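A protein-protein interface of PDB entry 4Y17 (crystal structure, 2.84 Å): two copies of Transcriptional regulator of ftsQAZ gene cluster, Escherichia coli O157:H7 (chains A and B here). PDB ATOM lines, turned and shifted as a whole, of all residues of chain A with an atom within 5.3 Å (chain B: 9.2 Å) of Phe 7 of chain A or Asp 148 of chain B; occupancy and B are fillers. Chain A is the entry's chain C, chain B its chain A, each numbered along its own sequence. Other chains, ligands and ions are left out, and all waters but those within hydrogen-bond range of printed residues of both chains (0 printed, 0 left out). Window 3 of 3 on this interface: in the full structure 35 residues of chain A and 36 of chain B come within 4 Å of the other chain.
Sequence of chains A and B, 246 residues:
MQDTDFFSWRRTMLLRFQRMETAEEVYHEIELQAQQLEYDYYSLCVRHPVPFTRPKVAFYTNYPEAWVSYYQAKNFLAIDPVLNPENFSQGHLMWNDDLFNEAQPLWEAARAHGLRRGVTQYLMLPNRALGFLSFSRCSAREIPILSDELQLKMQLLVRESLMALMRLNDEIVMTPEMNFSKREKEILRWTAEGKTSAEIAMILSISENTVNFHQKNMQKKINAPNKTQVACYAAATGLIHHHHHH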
ATOM      1  N   ASP A   3      10.680  17.791 -10.158  1.00  0.00           N
ATOM      2  CA  ASP A   3       9.477  17.470 -10.915  1.00  0.00           C
ATOM      3  C   ASP A   3       8.330  17.292  -9.936  1.00  0.00           C
ATOM      4  O   ASP A   3       7.250  17.849 -10.119  1.00  0.00           O
ATOM      5  CB  ASP A   3       9.666  16.201 -11.751  1.00  0.00           C
ATOM      6  CG  ASP A   3      10.725  16.359 -12.826  1.00  0.00           C
ATOM      7  OD1 ASP A   3      11.594  17.245 -12.682  1.00  0.00           O
ATOM      8  OD2 ASP A   3      10.691  15.594 -13.813  1.00  0.00           O
ATOM      9  N   THR A   4       8.593  16.533  -8.877  1.00  0.00           N
ATOM     10  CA  THR A   4       7.584  16.223  -7.873  1.00  0.00           C
ATOM     11  C   THR A   4       7.135  17.452  -7.085  1.00  0.00           C
ATOM     12  O   THR A   4       5.946  17.605  -6.804  1.00  0.00           O
ATOM     13  CB  THR A   4       8.096  15.163  -6.886  1.00  0.00           C
ATOM     14  OG1 THR A   4       9.386  15.545  -6.393  1.00  0.00           O
ATOM     15  CG2 THR A   4       8.198  13.811  -7.570  1.00  0.00           C
ATOM     16  N   ASP A   5       8.072  18.329  -6.729  1.00  0.00           N
ATOM     17  CA  ASP A   5       7.717  19.486  -5.914  1.00  0.00           C
ATOM     18  C   ASP A   5       6.998  20.544  -6.743  1.00  0.00           C
ATOM     19  O   ASP A   5       6.514  21.539  -6.204  1.00  0.00           O
ATOM     20  CB  ASP A   5       8.968  20.089  -5.264  1.00  0.00           C
ATOM     21  CG  ASP A   5       8.635  21.064  -4.146  1.00  0.00           C
ATOM     22  OD1 ASP A   5       7.842  20.698  -3.252  1.00  0.00           O
ATOM     23  OD2 ASP A   5       9.163  22.196  -4.160  1.00  0.00           O
ATOM     24  N   PHE A   6       6.913  20.324  -8.052  1.00  0.00           N
ATOM     25  CA  PHE A   6       6.085  21.169  -8.900  1.00  0.00           C
ATOM     26  C   PHE A   6       4.620  20.748  -8.804  1.00  0.00           C
ATOM     27  O   PHE A   6       3.731  21.594  -8.698  1.00  0.00           O
ATOM     28  CB  PHE A   6       6.564  21.116 -10.353  1.00  0.00           C
ATOM     29  CG  PHE A   6       5.590  21.703 -11.332  1.00  0.00           C
ATOM     30  CD1 PHE A   6       4.559  20.937 -11.853  1.00  0.00           C
ATOM     31  CD2 PHE A   6       5.705  23.022 -11.734  1.00  0.00           C
ATOM     32  CE1 PHE A   6       3.660  21.475 -12.749  1.00  0.00           C
ATOM     33  CE2 PHE A   6       4.810  23.567 -12.632  1.00  0.00           C
ATOM     34  CZ  PHE A   6       3.786  22.791 -13.141  1.00  0.00           C
ATOM     35  N   PHE A   7       4.372  19.439  -8.855  1.00  0.00           N
ATOM     36  CA  PHE A   7       3.008  18.920  -8.777  1.00  0.00           C
ATOM     37  C   PHE A   7       2.334  19.314  -7.478  1.00  0.00           C
ATOM     38  O   PHE A   7       1.149  19.622  -7.456  1.00  0.00           O
ATOM     39  CB  PHE A   7       2.990  17.392  -8.900  1.00  0.00           C
ATOM     40  CG  PHE A   7       3.548  16.868 -10.192  1.00  0.00           C
ATOM     41  CD1 PHE A   7       2.801  16.927 -11.356  1.00  0.00           C
ATOM     42  CD2 PHE A   7       4.814  16.323 -10.246  1.00  0.00           C
ATOM     43  CE1 PHE A   7       3.306  16.442 -12.548  1.00  0.00           C
ATOM     44  CE2 PHE A   7       5.330  15.840 -11.433  1.00  0.00           C
ATOM     45  CZ  PHE A   7       4.575  15.902 -12.586  1.00  0.00           C
ATOM     46  N   SER A   8       3.105  19.340  -6.400  1.00  0.00           N
ATOM     47  CA  SER A   8       2.570  19.713  -5.102  1.00  0.00           C
ATOM     48  C   SER A   8       2.372  21.213  -5.018  1.00  0.00           C
ATOM     49  O   SER A   8       1.469  21.691  -4.334  1.00  0.00           O
ATOM     50  CB  SER A   8       3.485  19.236  -3.981  1.00  0.00           C
ATOM     51  OG  SER A   8       4.782  19.793  -4.099  1.00  0.00           O
ATOM     52  N   TRP A   9       3.202  21.956  -5.738  1.00  0.00           N
ATOM     53  CA  TRP A   9       3.033  23.394  -5.789  1.00  0.00           C
ATOM     54  C   TRP A   9       1.663  23.643  -6.395  1.00  0.00           C
ATOM     55  O   TRP A   9       0.875  24.399  -5.844  1.00  0.00           O
ATOM     56  CB  TRP A   9       4.139  24.067  -6.606  1.00  0.00           C
ATOM     57  CG  TRP A   9       4.011  25.559  -6.675  1.00  0.00           C
ATOM     58  CD1 TRP A   9       4.490  26.463  -5.769  1.00  0.00           C
ATOM     59  CD2 TRP A   9       3.360  26.325  -7.696  1.00  0.00           C
ATOM     60  NE1 TRP A   9       4.181  27.740  -6.165  1.00  0.00           N
ATOM     61  CE2 TRP A   9       3.488  27.684  -7.345  1.00  0.00           C
ATOM     62  CE3 TRP A   9       2.687  25.994  -8.874  1.00  0.00           C
ATOM     63  CZ2 TRP A   9       2.966  28.710  -8.129  1.00  0.00           C
ATOM     64  CZ3 TRP A   9       2.169  27.016  -9.649  1.00  0.00           C
ATOM     65  CH2 TRP A   9       2.312  28.356  -9.275  1.00  0.00           C
ATOM     66  N   ARG A  10       1.356  22.950  -7.489  1.00  0.00           N
ATOM     67  CA  ARG A  10       0.050  23.083  -8.127  1.00  0.00           C
ATOM     68  C   ARG A  10      -1.090  22.777  -7.171  1.00  0.00           C
ATOM     69  O   ARG A  10      -2.056  23.534  -7.078  1.00  0.00           O
ATOM     70  CB  ARG A  10      -0.098  22.129  -9.315  1.00  0.00           C
ATOM     71  CG  ARG A  10      -1.446  22.287 -10.031  1.00  0.00           C
ATOM     72  CD  ARG A  10      -1.841  21.112 -10.895  1.00  0.00           C
ATOM     73  NE  ARG A  10      -0.721  20.337 -11.408  1.00  0.00           N
ATOM     74  CZ  ARG A  10      -0.849  19.122 -11.930  1.00  0.00           C
ATOM     75  NH1 ARG A  10      -2.044  18.550 -11.999  1.00  0.00           N
ATOM     76  NH2 ARG A  10       0.216  18.474 -12.377  1.00  0.00           N
ATOM     77  N   ARG A  11      -0.963  21.660  -6.463  1.00  0.00           N
ATOM     78  CA  ARG A  11      -2.052  21.149  -5.647  1.00  0.00           C
ATOM     79  C   ARG A  11      -2.390  22.164  -4.568  1.00  0.00           C
ATOM     80  O   ARG A  11      -3.555  22.382  -4.266  1.00  0.00           O
ATOM     81  CB  ARG A  11      -1.670  19.786  -5.059  1.00  0.00           C
ATOM     82  CG  ARG A  11      -1.535  18.739  -6.161  1.00  0.00           C
ATOM     83  CD  ARG A  11      -0.903  17.421  -5.732  1.00  0.00           C
ATOM     84  NE  ARG A  11      -1.881  16.380  -5.431  1.00  0.00           N
ATOM     85  CZ  ARG A  11      -1.565  15.144  -5.053  1.00  0.00           C
ATOM     86  NH1 ARG A  11      -0.295  14.787  -4.922  1.00  0.00           N
ATOM     87  NH2 ARG A  11      -2.519  14.254  -4.816  1.00  0.00           N
ATOM     88  N   ASP B   5      13.131  15.970 -16.260  1.00  0.00           N
ATOM     89  CA  ASP B   5      13.078  14.831 -17.168  1.00  0.00           C
ATOM     90  C   ASP B   5      11.689  14.690 -17.786  1.00  0.00           C
ATOM     91  O   ASP B   5      11.547  14.199 -18.906  1.00  0.00           O
ATOM     92  CB  ASP B   5      13.458  13.545 -16.432  1.00  0.00           C
ATOM     93  CG  ASP B   5      13.740  12.390 -17.375  1.00  0.00           C
ATOM     94  OD1 ASP B   5      12.778  11.694 -17.765  1.00  0.00           O
ATOM     95  OD2 ASP B   5      14.921  12.175 -17.723  1.00  0.00           O
ATOM     96  N   PHE B   6      10.670  15.134 -17.056  1.00  0.00           N
ATOM     97  CA  PHE B   6       9.317  15.212 -17.596  1.00  0.00           C
ATOM     98  C   PHE B   6       9.230  16.394 -18.550  1.00  0.00           C
ATOM     99  O   PHE B   6       8.601  16.315 -19.603  1.00  0.00           O
ATOM    100  CB  PHE B   6       8.285  15.354 -16.472  1.00  0.00           C
ATOM    101  CG  PHE B   6       6.913  15.763 -16.948  1.00  0.00           C
ATOM    102  CD1 PHE B   6       6.632  17.084 -17.261  1.00  0.00           C
ATOM    103  CD2 PHE B   6       5.900  14.826 -17.068  1.00  0.00           C
ATOM    104  CE1 PHE B   6       5.377  17.461 -17.697  1.00  0.00           C
ATOM    105  CE2 PHE B   6       4.639  15.198 -17.501  1.00  0.00           C
ATOM    106  CZ  PHE B   6       4.379  16.517 -17.814  1.00  0.00           C
ATOM    107  N   PHE B   7       9.855  17.499 -18.159  1.00  0.00           N
ATOM    108  CA  PHE B   7       9.851  18.715 -18.960  1.00  0.00           C
ATOM    109  C   PHE B   7      10.430  18.436 -20.346  1.00  0.00           C
ATOM    110  O   PHE B   7      10.074  19.103 -21.318  1.00  0.00           O
ATOM    111  CB  PHE B   7      10.616  19.833 -18.241  1.00  0.00           C
ATOM    112  CG  PHE B   7      10.066  20.165 -16.871  1.00  0.00           C
ATOM    113  CD1 PHE B   7       8.787  19.770 -16.507  1.00  0.00           C
ATOM    114  CD2 PHE B   7      10.820  20.881 -15.955  1.00  0.00           C
ATOM    115  CE1 PHE B   7       8.275  20.071 -15.259  1.00  0.00           C
ATOM    116  CE2 PHE B   7      10.310  21.185 -14.701  1.00  0.00           C
ATOM    117  CZ  PHE B   7       9.036  20.779 -14.355  1.00  0.00           C
ATOM    118  N   TRP B   9       9.973  15.569 -21.880  1.00  0.00           N
ATOM    119  CA  TRP B   9       8.862  14.904 -22.564  1.00  0.00           C
ATOM    120  C   TRP B   9       7.913  15.929 -23.168  1.00  0.00           C
ATOM    121  O   TRP B   9       7.499  15.800 -24.320  1.00  0.00           O
ATOM    122  CB  TRP B   9       8.090  13.983 -21.615  1.00  0.00           C
ATOM    123  CG  TRP B   9       6.899  13.333 -22.260  1.00  0.00           C
ATOM    124  CD1 TRP B   9       6.885  12.185 -22.995  1.00  0.00           C
ATOM    125  CD2 TRP B   9       5.542  13.799 -22.219  1.00  0.00           C
ATOM    126  NE1 TRP B   9       5.606  11.908 -23.418  1.00  0.00           N
ATOM    127  CE2 TRP B   9       4.763  12.883 -22.953  1.00  0.00           C
ATOM    128  CE3 TRP B   9       4.912  14.903 -21.632  1.00  0.00           C
ATOM    129  CZ2 TRP B   9       3.386  13.035 -23.116  1.00  0.00           C
ATOM    130  CZ3 TRP B   9       3.546  15.052 -21.798  1.00  0.00           C
ATOM    131  CH2 TRP B   9       2.799  14.124 -22.533  1.00  0.00           C
ATOM    132  N   GLN B  90     -10.667  20.068 -13.173  1.00  0.00           N
ATOM    133  CA  GLN B  90      -9.425  20.474 -13.824  1.00  0.00           C
ATOM    134  C   GLN B  90      -9.353  19.869 -15.226  1.00  0.00           C
ATOM    135  O   GLN B  90      -8.271  19.615 -15.755  1.00  0.00           O
ATOM    136  CB  GLN B  90      -8.199  20.064 -13.006  1.00  0.00           C
ATOM    137  CG  GLN B  90      -6.962  20.900 -13.327  1.00  0.00           C
ATOM    138  CD  GLN B  90      -5.673  20.270 -12.839  1.00  0.00           C
ATOM    139  OE1 GLN B  90      -5.685  19.361 -12.008  1.00  0.00           O
ATOM    140  NE2 GLN B  90      -4.549  20.749 -13.360  1.00  0.00           N
ATOM    141  N   HIS B  92     -10.207  16.917 -16.072  1.00  0.00           N
ATOM    142  CA  HIS B  92      -9.793  15.519 -16.001  1.00  0.00           C
ATOM    143  C   HIS B  92     -10.901  14.661 -15.403  1.00  0.00           C
ATOM    144  O   HIS B  92     -11.729  15.149 -14.630  1.00  0.00           O
ATOM    145  CB  HIS B  92      -8.518  15.374 -15.173  1.00  0.00           C
ATOM    146  CG  HIS B  92      -7.985  13.976 -15.130  1.00  0.00           C
ATOM    147  ND1 HIS B  92      -7.062  13.504 -16.040  1.00  0.00           N
ATOM    148  CD2 HIS B  92      -8.243  12.947 -14.289  1.00  0.00           C
ATOM    149  CE1 HIS B  92      -6.773  12.246 -15.759  1.00  0.00           C
ATOM    150  NE2 HIS B  92      -7.478  11.883 -14.703  1.00  0.00           N
ATOM    151  N   MET B  94     -11.491  10.362 -14.190  1.00  0.00           N
ATOM    152  CA  MET B  94     -11.151   8.947 -14.090  1.00  0.00           C
ATOM    153  C   MET B  94     -12.453   8.155 -14.111  1.00  0.00           C
ATOM    154  O   MET B  94     -13.404   8.503 -13.412  1.00  0.00           O
ATOM    155  CB  MET B  94     -10.358   8.662 -12.814  1.00  0.00           C
ATOM    156  CG  MET B  94      -9.895   7.217 -12.666  1.00  0.00           C
ATOM    157  SD  MET B  94      -8.558   6.793 -13.799  1.00  0.00           S
ATOM    158  CE  MET B  94      -7.195   7.712 -13.083  1.00  0.00           C
ATOM    159  N   GLN B 121      -9.640  13.247 -20.692  1.00  0.00           N
ATOM    160  CA  GLN B 121      -9.230  14.641 -20.530  1.00  0.00           C
ATOM    161  C   GLN B 121      -9.986  15.501 -21.549  1.00  0.00           C
ATOM    162  O   GLN B 121     -10.348  15.012 -22.619  1.00  0.00           O
ATOM    163  CB  GLN B 121      -7.718  14.784 -20.715  1.00  0.00           C
ATOM    164  CG  GLN B 121      -7.164  16.150 -20.331  1.00  0.00           C
ATOM    165  CD  GLN B 121      -7.124  16.360 -18.827  1.00  0.00           C
ATOM    166  OE1 GLN B 121      -7.019  15.406 -18.057  1.00  0.00           O
ATOM    167  NE2 GLN B 121      -7.219  17.613 -18.401  1.00  0.00           N
ATOM    168  N   ILE B 145       0.802   4.444 -12.554  1.00  0.00           N
ATOM    169  CA  ILE B 145       0.931   5.874 -12.815  1.00  0.00           C
ATOM    170  C   ILE B 145       0.732   6.678 -11.534  1.00  0.00           C
ATOM    171  O   ILE B 145      -0.048   6.290 -10.667  1.00  0.00           O
ATOM    172  CB  ILE B 145      -0.096   6.347 -13.861  1.00  0.00           C
ATOM    173  N   LEU B 146       1.442   7.797 -11.418  1.00  0.00           N
ATOM    174  CA  LEU B 146       0.879   8.985 -10.787  1.00  0.00           C
ATOM    175  C   LEU B 146      -0.282   9.532 -11.611  1.00  0.00           C
ATOM    176  O   LEU B 146      -0.195   9.635 -12.835  1.00  0.00           O
ATOM    177  CB  LEU B 146       1.954  10.061 -10.625  1.00  0.00           C
ATOM    178  CG  LEU B 146       1.688  11.100  -9.534  1.00  0.00           C
ATOM    179  CD1 LEU B 146       1.204  10.426  -8.258  1.00  0.00           C
ATOM    180  CD2 LEU B 146       2.936  11.927  -9.265  1.00  0.00           C
ATOM    181  N   SER B 147      -1.368   9.882 -10.930  1.00  0.00           N
ATOM    182  CA  SER B 147      -2.450  10.658 -11.531  1.00  0.00           C
ATOM    183  C   SER B 147      -2.036  12.062 -11.962  1.00  0.00           C
ATOM    184  O   SER B 147      -2.420  12.519 -13.033  1.00  0.00           O
ATOM    185  CB  SER B 147      -3.619  10.769 -10.550  1.00  0.00           C
ATOM    186  OG  SER B 147      -3.340  11.714  -9.530  1.00  0.00           O
ATOM    187  N   ASP B 148      -1.248  12.738 -11.135  1.00  0.00           N
ATOM    188  CA  ASP B 148      -0.785  14.083 -11.456  1.00  0.00           C
ATOM    189  C   ASP B 148       0.007  14.128 -12.759  1.00  0.00           C
ATOM    190  O   ASP B 148      -0.180  15.032 -13.573  1.00  0.00           O
ATOM    191  CB  ASP B 148       0.066  14.627 -10.316  1.00  0.00           C
ATOM    192  CG  ASP B 148      -0.771  15.184  -9.189  1.00  0.00           C
ATOM    193  OD1 ASP B 148      -1.919  14.724  -9.010  1.00  0.00           O
ATOM    194  OD2 ASP B 148      -0.283  16.087  -8.488  1.00  0.00           O
ATOM    195  N   GLU B 149       0.886  13.154 -12.958  1.00  0.00           N
ATOM    196  CA  GLU B 149       1.661  13.093 -14.187  1.00  0.00           C
ATOM    197  C   GLU B 149       0.741  12.644 -15.317  1.00  0.00           C
ATOM    198  O   GLU B 149       0.949  12.994 -16.477  1.00  0.00           O
ATOM    199  CB  GLU B 149       2.854  12.148 -14.043  1.00  0.00           C
ATOM    200  CG  GLU B 149       3.866  12.263 -15.173  1.00  0.00           C
ATOM    201  CD  GLU B 149       4.920  11.174 -15.132  1.00  0.00           C
ATOM    202  OE1 GLU B 149       4.562  10.002 -14.885  1.00  0.00           O
ATOM    203  OE2 GLU B 149       6.110  11.492 -15.343  1.00  0.00           O
ATOM    204  N   LEU B 150      -0.283  11.870 -14.969  1.00  0.00           N
ATOM    205  CA  LEU B 150      -1.263  11.418 -15.947  1.00  0.00           C
ATOM    206  C   LEU B 150      -2.115  12.586 -16.422  1.00  0.00           C
ATOM    207  O   LEU B 150      -2.268  12.800 -17.625  1.00  0.00           O
ATOM    208  CB  LEU B 150      -2.167  10.330 -15.362  1.00  0.00           C
ATOM    209  CG  LEU B 150      -3.157   9.709 -16.353  1.00  0.00           C
ATOM    210  CD1 LEU B 150      -2.430   8.849 -17.378  1.00  0.00           C
ATOM    211  CD2 LEU B 150      -4.237   8.916 -15.629  1.00  0.00           C
ATOM    212  N   GLN B 151      -2.681  13.328 -15.470  1.00  0.00           N
ATOM    213  CA  GLN B 151      -3.479  14.502 -15.793  1.00  0.00           C
ATOM    214  C   GLN B 151      -2.707  15.442 -16.703  1.00  0.00           C
ATOM    215  O   GLN B 151      -3.236  15.912 -17.705  1.00  0.00           O
ATOM    216  CB  GLN B 151      -3.903  15.256 -14.527  1.00  0.00           C
ATOM    217  CG  GLN B 151      -4.834  14.493 -13.595  1.00  0.00           C
ATOM    218  CD  GLN B 151      -5.304  15.334 -12.422  1.00  0.00           C
ATOM    219  OE1 GLN B 151      -5.293  16.563 -12.481  1.00  0.00           O
ATOM    220  NE2 GLN B 151      -5.732  14.672 -11.352  1.00  0.00           N
ATOM    221  N   LEU B 152      -1.449  15.690 -16.362  1.00  0.00           N
ATOM    222  CA  LEU B 152      -0.638  16.659 -17.089  1.00  0.00           C
ATOM    223  C   LEU B 152      -0.191  16.146 -18.454  1.00  0.00           C
ATOM    224  O   LEU B 152      -0.112  16.918 -19.411  1.00  0.00           O
ATOM    225  CB  LEU B 152       0.584  17.052 -16.259  1.00  0.00           C
ATOM    226  CG  LEU B 152       0.963  18.533 -16.342  1.00  0.00           C
ATOM    227  CD1 LEU B 152      -0.092  19.400 -15.666  1.00  0.00           C
ATOM    228  CD2 LEU B 152       2.332  18.779 -15.731  1.00  0.00           C
ATOM    229  N   LYS B 153       0.105  14.854 -18.549  1.00  0.00           N
ATOM    230  CA  LYS B 153       0.492  14.269 -19.828  1.00  0.00           C
ATOM    231  C   LYS B 153      -0.677  14.291 -20.811  1.00  0.00           C
ATOM    232  O   LYS B 153      -0.508  14.645 -21.977  1.00  0.00           O
ATOM    233  CB  LYS B 153       1.006  12.838 -19.643  1.00  0.00           C
ATOM    234  CG  LYS B 153       2.465  12.753 -19.204  1.00  0.00           C
ATOM    235  CD  LYS B 153       2.963  11.316 -19.153  1.00  0.00           C
ATOM    236  CE  LYS B 153       4.479  11.260 -19.032  1.00  0.00           C
ATOM    237  NZ  LYS B 153       5.013   9.876 -19.148  1.00  0.00           N
ATOM    238  N   MET B 154      -1.861  13.921 -20.336  1.00  0.00           N
ATOM    239  CA  MET B 154      -3.053  13.919 -21.177  1.00  0.00           C
ATOM    240  C   MET B 154      -3.482  15.339 -21.538  1.00  0.00           C
ATOM    241  O   MET B 154      -3.977  15.584 -22.638  1.00  0.00           O
ATOM    242  CB  MET B 154      -4.207  13.196 -20.481  1.00  0.00           C
ATOM    243  CG  MET B 154      -4.102  11.682 -20.504  1.00  0.00           C
ATOM    244  SD  MET B 154      -5.571  10.893 -19.821  1.00  0.00           S
ATOM    245  CE  MET B 154      -6.613  10.776 -21.272  1.00  0.00           C
ATOM    246  N   GLN B 155      -3.304  16.260 -20.595  1.00  0.00           N
ATOM    247  CA  GLN B 155      -3.623  17.671 -20.800  1.00  0.00           C
ATOM    248  C   GLN B 155      -2.942  18.192 -22.063  1.00  0.00           C
ATOM    249  O   GLN B 155      -3.555  18.891 -22.868  1.00  0.00           O
ATOM    250  CB  GLN B 155      -3.202  18.490 -19.579  1.00  0.00           C
ATOM    251  CG  GLN B 155      -3.996  19.761 -19.366  1.00  0.00           C
ATOM    252  CD  GLN B 155      -3.559  20.508 -18.119  1.00  0.00           C
ATOM    253  OE1 GLN B 155      -2.861  21.517 -18.198  1.00  0.00           O
ATOM    254  NE2 GLN B 155      -3.959  20.001 -16.955  1.00  0.00           N
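Positions printed for both chains: 5, 6, 7 and 9. Of the 8 pairs that touch across the chains among the printed residues, none has its exchanged pair printed and touching as well.
Phe 7 of chain A touches just one residue of chain B: Asp 148. Of chain A, only Phe 7 (3.5 Å), Arg 10 (3.7 Å) and Arg 11 (3.1 Å) come within 4 Å of Asp 148 of chain B. No residue of chain B comes within 4 Å of Ser 8 of chain A. Of chain B, only Gln 90, Asp 148, Gln 151 and Leu 152 come within 4 Å of Arg 10 of chain A. Of the printed residues of chain B, Arg 11 of chain A touches Asp 148 (3.1 Å). Printed residues of chain A within 4 Å of Asp 5 of chain B: Asp 3 (3.5 Å). Of the printed residues of chain B, Asp 3 of chain A touches Asp 5 (3.5 Å) and Phe 6 (3.3 Å). Of the printed residues of chain A, Gln 151 of chain B touches Arg 10. Lys 153 of chain B touches none of the printed residues of chain A.
Among the printed residues, pairs that only touch across the chains: Phe 7 of chain A with Asp 148 of chain B, Arg 10 of chain A with Gln 90 of chain B, Arg 10 of chain A with Asp 148 of chain B, Arg 10 of chain A with Gln 151 of chain B and Arg 10 of chain A with Leu 152 of chain B.
Printed residues of chain B that touch a printed residue of chain A: Asp 5, Phe 6, Gln 90, Asp 148, Gln 151 and Leu 152. Of the 9 printed residues of chain A, 4 touch a printed residue of chain B. Hydrophobic or aromatic side chains of chain A within 4 Å of the printed part of chain B: Phe 7. Among the printed residues, Asp or Glu carboxylates within 4 Å of a Lys or Arg side-chain nitrogen of the other chain: Arg 11 of chain A with Asp 148 of chain B (3.5 Å).
NE2 of Gln 121 of chain B sits at hydrogen-bond distance from O of Gln 90 of chain B, at 3.5 Å. The side-chain amide oxygen (OE1) of Gln 90 of chain B sits close to the side-chain amide oxygen (OE1) of Gln 151 of chain B (2.9 Å). OD1 of Asp 148 of chain B sits at hydrogen-bond distance from OG of Ser 147 of chain B (3.4 Å).
The backbone NH (N) of Asp 5 of chain B sits at hydrogen-bond distance from the side-chain carboxylate (OD2) of Asp 3 of chain A (3.5 Å). The side-chain carboxylate (OD2) of Asp 3 of chain A sits at hydrogen-bond distance from the backbone NH (N) of Phe 6 of chain B, 3.3 Å away. OD2 of Asp 148 of chain B lies within salt-bridge range of NE of Arg 11 of chain A, at 3.5 Å.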
